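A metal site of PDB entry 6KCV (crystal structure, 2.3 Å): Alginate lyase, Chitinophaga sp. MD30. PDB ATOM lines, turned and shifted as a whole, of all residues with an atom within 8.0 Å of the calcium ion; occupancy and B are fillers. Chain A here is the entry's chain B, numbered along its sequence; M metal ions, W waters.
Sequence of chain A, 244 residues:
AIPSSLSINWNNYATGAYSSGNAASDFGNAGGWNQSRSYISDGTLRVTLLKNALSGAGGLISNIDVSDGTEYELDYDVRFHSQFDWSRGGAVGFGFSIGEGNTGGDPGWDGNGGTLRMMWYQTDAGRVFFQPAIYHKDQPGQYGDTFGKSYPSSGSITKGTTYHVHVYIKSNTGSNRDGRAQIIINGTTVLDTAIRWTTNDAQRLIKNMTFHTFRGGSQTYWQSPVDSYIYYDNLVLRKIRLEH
Within 4 Å of the calcium ion: Asn 9, Asn 11, Gly 43 and Asp 233.
The backbone carbonyl oxygen (O) of Asp 233 lies within hydrogen-bond range of the backbone NH (N) of Asp 77 (2.9 Å). OD1 of Asp 233 lies close to OD1 of Asn 234, at 3.5 Å.
The calcium ion is bound by O of Gly 43 (2.3 Å), O of Asn 9 (2.3 Å), water W2 (2.5 Å), water W1 (2.5 Å), OD2 of Asp 233 (2.5 Å), OD1 of Asn 11 (2.5 Å) and OD1 of Asp 233 (2.6 Å). The calcium ion has seven donor atoms within binding distance.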
ATOM      1  N   ILE A   8      -4.727 -12.216  -7.711  1.00  0.00           N
ATOM      2  CA  ILE A   8      -4.847 -11.549  -9.002  1.00  0.00           C
ATOM      3  C   ILE A   8      -5.660 -12.440  -9.920  1.00  0.00           C
ATOM      4  O   ILE A   8      -5.294 -13.608 -10.120  1.00  0.00           O
ATOM      5  CB  ILE A   8      -3.475 -11.242  -9.629  1.00  0.00           C
ATOM      6  CG1 ILE A   8      -2.567 -10.497  -8.656  1.00  0.00           C
ATOM      7  CG2 ILE A   8      -3.664 -10.468 -10.927  1.00  0.00           C
ATOM      8  CD1 ILE A   8      -1.106 -10.381  -9.135  1.00  0.00           C
ATOM      9  N   ASN A   9      -6.737 -11.908 -10.502  1.00  0.00           N
ATOM     10  CA  ASN A   9      -7.511 -12.681 -11.458  1.00  0.00           C
ATOM     11  C   ASN A   9      -7.643 -12.018 -12.829  1.00  0.00           C
ATOM     12  O   ASN A   9      -8.274 -12.597 -13.723  1.00  0.00           O
ATOM     13  CB  ASN A   9      -8.901 -12.994 -10.878  1.00  0.00           C
ATOM     14  CG  ASN A   9      -9.711 -11.742 -10.560  1.00  0.00           C
ATOM     15  OD1 ASN A   9      -9.629 -10.733 -11.263  1.00  0.00           O
ATOM     16  ND2 ASN A   9     -10.492 -11.815  -9.491  1.00  0.00           N
ATOM     17  N   TRP A  10      -7.069 -10.828 -13.029  1.00  0.00           N
ATOM     18  CA  TRP A  10      -7.092 -10.107 -14.303  1.00  0.00           C
ATOM     19  C   TRP A  10      -8.507  -9.861 -14.819  1.00  0.00           C
ATOM     20  O   TRP A  10      -8.694  -9.594 -16.022  1.00  0.00           O
ATOM     21  CB  TRP A  10      -6.232 -10.838 -15.356  1.00  0.00           C
ATOM     22  CG  TRP A  10      -4.789 -10.814 -14.953  1.00  0.00           C
ATOM     23  CD1 TRP A  10      -3.930  -9.751 -15.075  1.00  0.00           C
ATOM     24  CD2 TRP A  10      -4.061 -11.856 -14.307  1.00  0.00           C
ATOM     25  NE1 TRP A  10      -2.706 -10.088 -14.553  1.00  0.00           N
ATOM     26  CE2 TRP A  10      -2.750 -11.375 -14.073  1.00  0.00           C
ATOM     27  CE3 TRP A  10      -4.362 -13.158 -13.916  1.00  0.00           C
ATOM     28  CZ2 TRP A  10      -1.769 -12.136 -13.469  1.00  0.00           C
ATOM     29  CZ3 TRP A  10      -3.389 -13.914 -13.317  1.00  0.00           C
ATOM     30  CH2 TRP A  10      -2.101 -13.404 -13.101  1.00  0.00           C
ATOM     31  N   ASN A  11      -9.519  -9.913 -13.959  1.00  0.00           N
ATOM     32  CA  ASN A  11     -10.909  -9.864 -14.433  1.00  0.00           C
ATOM     33  C   ASN A  11     -11.369  -8.448 -14.752  1.00  0.00           C
ATOM     34  O   ASN A  11     -12.361  -8.282 -15.462  1.00  0.00           O
ATOM     35  CB  ASN A  11     -11.851 -10.505 -13.411  1.00  0.00           C
ATOM     36  CG  ASN A  11     -11.840 -12.025 -13.479  1.00  0.00           C
ATOM     37  OD1 ASN A  11     -11.309 -12.598 -14.423  1.00  0.00           O
ATOM     38  ND2 ASN A  11     -12.435 -12.681 -12.487  1.00  0.00           N
ATOM     39  N   ASN A  12     -10.666  -7.439 -14.271  1.00  0.00           N
ATOM     40  CA  ASN A  12     -11.059  -6.047 -14.406  1.00  0.00           C
ATOM     41  C   ASN A  12     -10.563  -5.426 -15.691  1.00  0.00           C
ATOM     42  O   ASN A  12     -10.833  -4.246 -15.950  1.00  0.00           O
ATOM     43  CB  ASN A  12     -10.517  -5.239 -13.217  1.00  0.00           C
ATOM     44  CG  ASN A  12      -9.014  -5.503 -12.992  1.00  0.00           C
ATOM     45  OD1 ASN A  12      -8.601  -6.661 -12.836  1.00  0.00           O
ATOM     46  ND2 ASN A  12      -8.203  -4.445 -12.992  1.00  0.00           N
ATOM     47  N   ILE A  40      -4.014  -9.339 -22.119  1.00  0.00           N
ATOM     48  CA  ILE A  40      -5.198  -9.856 -21.442  1.00  0.00           C
ATOM     49  C   ILE A  40      -6.103 -10.474 -22.498  1.00  0.00           C
ATOM     50  O   ILE A  40      -6.507  -9.803 -23.458  1.00  0.00           O
ATOM     51  CB  ILE A  40      -5.926  -8.758 -20.657  1.00  0.00           C
ATOM     52  CG1 ILE A  40      -5.022  -8.212 -19.571  1.00  0.00           C
ATOM     53  CG2 ILE A  40      -7.158  -9.340 -19.978  1.00  0.00           C
ATOM     54  CD1 ILE A  40      -4.462  -9.297 -18.688  1.00  0.00           C
ATOM     55  N   SER A  41      -6.408 -11.745 -22.322  1.00  0.00           N
ATOM     56  CA  SER A  41      -7.264 -12.471 -23.243  1.00  0.00           C
ATOM     57  C   SER A  41      -8.421 -13.036 -22.415  1.00  0.00           C
ATOM     58  O   SER A  41      -8.258 -14.056 -21.750  1.00  0.00           O
ATOM     59  CB  SER A  41      -6.465 -13.562 -23.954  1.00  0.00           C
ATOM     60  OG  SER A  41      -7.248 -14.203 -24.944  1.00  0.00           O
ATOM     61  N   ASP A  42      -9.568 -12.346 -22.422  1.00  0.00           N
ATOM     62  CA  ASP A  42     -10.790 -12.852 -21.782  1.00  0.00           C
ATOM     63  C   ASP A  42     -10.569 -13.163 -20.295  1.00  0.00           C
ATOM     64  O   ASP A  42     -10.709 -14.298 -19.837  1.00  0.00           O
ATOM     65  CB  ASP A  42     -11.310 -14.074 -22.560  1.00  0.00           C
ATOM     66  CG  ASP A  42     -12.626 -14.621 -21.997  1.00  0.00           C
ATOM     67  OD1 ASP A  42     -13.508 -13.810 -21.632  1.00  0.00           O
ATOM     68  OD2 ASP A  42     -12.763 -15.867 -21.940  1.00  0.00           O
ATOM     69  N   GLY A  43     -10.185 -12.133 -19.545  1.00  0.00           N
ATOM     70  CA  GLY A  43      -9.953 -12.268 -18.116  1.00  0.00           C
ATOM     71  C   GLY A  43      -8.772 -13.131 -17.749  1.00  0.00           C
ATOM     72  O   GLY A  43      -8.678 -13.621 -16.616  1.00  0.00           O
ATOM     73  N   THR A  44      -7.826 -13.284 -18.678  1.00  0.00           N
ATOM     74  CA  THR A  44      -6.700 -14.186 -18.568  1.00  0.00           C
ATOM     75  C   THR A  44      -5.449 -13.433 -18.999  1.00  0.00           C
ATOM     76  O   THR A  44      -5.512 -12.602 -19.905  1.00  0.00           O
ATOM     77  CB  THR A  44      -6.976 -15.396 -19.471  1.00  0.00           C
ATOM     78  OG1 THR A  44      -7.893 -16.306 -18.825  1.00  0.00           O
ATOM     79  CG2 THR A  44      -5.731 -16.065 -19.936  1.00  0.00           C
ATOM     80  N   LEU A  45      -4.317 -13.709 -18.338  1.00  0.00           N
ATOM     81  CA  LEU A  45      -3.040 -13.130 -18.747  1.00  0.00           C
ATOM     82  C   LEU A  45      -2.337 -14.048 -19.735  1.00  0.00           C
ATOM     83  O   LEU A  45      -1.915 -15.165 -19.380  1.00  0.00           O
ATOM     84  CB  LEU A  45      -2.134 -12.853 -17.550  1.00  0.00           C
ATOM     85  CG  LEU A  45      -0.722 -12.350 -17.911  1.00  0.00           C
ATOM     86  CD1 LEU A  45      -0.775 -11.045 -18.672  1.00  0.00           C
ATOM     87  CD2 LEU A  45       0.174 -12.240 -16.671  1.00  0.00           C
ATOM     88  N   ASP A  77      -3.452 -21.077 -12.159  1.00  0.00           N
ATOM     89  CA  ASP A  77      -3.858 -21.895 -13.292  1.00  0.00           C
ATOM     90  C   ASP A  77      -2.996 -21.572 -14.497  1.00  0.00           C
ATOM     91  O   ASP A  77      -2.737 -20.402 -14.790  1.00  0.00           O
ATOM     92  CB  ASP A  77      -5.327 -21.629 -13.643  1.00  0.00           C
ATOM     93  CG  ASP A  77      -6.238 -22.018 -12.526  1.00  0.00           C
ATOM     94  OD1 ASP A  77      -6.117 -23.166 -12.044  1.00  0.00           O
ATOM     95  OD2 ASP A  77      -7.048 -21.177 -12.107  1.00  0.00           O
ATOM     96  N   TYR A 232      -2.360 -17.674 -18.146  1.00  0.00           N
ATOM     97  CA  TYR A 232      -2.312 -17.758 -16.689  1.00  0.00           C
ATOM     98  C   TYR A 232      -3.564 -17.136 -16.083  1.00  0.00           C
ATOM     99  O   TYR A 232      -4.140 -16.201 -16.631  1.00  0.00           O
ATOM    100  CB  TYR A 232      -1.083 -17.025 -16.145  1.00  0.00           C
ATOM    101  CG  TYR A 232       0.246 -17.615 -16.586  1.00  0.00           C
ATOM    102  CD1 TYR A 232       0.789 -18.713 -15.925  1.00  0.00           C
ATOM    103  CD2 TYR A 232       0.945 -17.084 -17.654  1.00  0.00           C
ATOM    104  CE1 TYR A 232       1.991 -19.241 -16.304  1.00  0.00           C
ATOM    105  CE2 TYR A 232       2.155 -17.622 -18.060  1.00  0.00           C
ATOM    106  CZ  TYR A 232       2.674 -18.695 -17.371  1.00  0.00           C
ATOM    107  OH  TYR A 232       3.870 -19.243 -17.744  1.00  0.00           O
ATOM    108  N   ASP A 233      -3.969 -17.630 -14.913  1.00  0.00           N
ATOM    109  CA  ASP A 233      -5.103 -17.037 -14.218  1.00  0.00           C
ATOM    110  C   ASP A 233      -5.046 -17.371 -12.734  1.00  0.00           C
ATOM    111  O   ASP A 233      -4.432 -18.362 -12.321  1.00  0.00           O
ATOM    112  CB  ASP A 233      -6.452 -17.475 -14.826  1.00  0.00           C
ATOM    113  CG  ASP A 233      -7.545 -16.422 -14.665  1.00  0.00           C
ATOM    114  OD1 ASP A 233      -7.329 -15.471 -13.885  1.00  0.00           O
ATOM    115  OD2 ASP A 233      -8.610 -16.550 -15.308  1.00  0.00           O
ATOM    116  N   ASN A 234      -5.684 -16.515 -11.937  1.00  0.00           N
ATOM    117  CA  ASN A 234      -5.977 -16.822 -10.520  1.00  0.00           C
ATOM    118  C   ASN A 234      -4.703 -17.044  -9.707  1.00  0.00           C
ATOM    119  O   ASN A 234      -4.540 -18.063  -9.042  1.00  0.00           O
ATOM    120  CB  ASN A 234      -6.917 -18.018 -10.423  1.00  0.00           C
ATOM    121  CG  ASN A 234      -8.191 -17.819 -11.216  1.00  0.00           C
ATOM    122  OD1 ASN A 234      -8.873 -16.815 -11.050  1.00  0.00           O
ATOM    123  ND2 ASN A 234      -8.510 -18.757 -12.108  1.00  0.00           N
ATOM    124  N   LEU A 235      -3.798 -16.083  -9.752  1.00  0.00           N
ATOM    125  CA  LEU A 235      -2.599 -16.177  -8.935  1.00  0.00           C
ATOM    126  C   LEU A 235      -2.952 -15.783  -7.509  1.00  0.00           C
ATOM    127  O   LEU A 235      -3.407 -14.653  -7.275  1.00  0.00           O
ATOM    128  CB  LEU A 235      -1.488 -15.274  -9.455  1.00  0.00           C
ATOM    129  CG  LEU A 235      -0.400 -15.308  -8.370  1.00  0.00           C
ATOM    130  CD1 LEU A 235       0.556 -16.514  -8.554  1.00  0.00           C
ATOM    131  CD2 LEU A 235       0.360 -13.986  -8.213  1.00  0.00           C
HETATM  132 CA    CA M   1      -9.529 -14.342 -14.653  1.00  0.00          CA
HETATM  133  O   HOH W   1     -11.356 -15.161 -16.104  1.00  0.00           O
HETATM  134  O   HOH W   2     -10.429 -15.558 -12.703  1.00  0.00           O
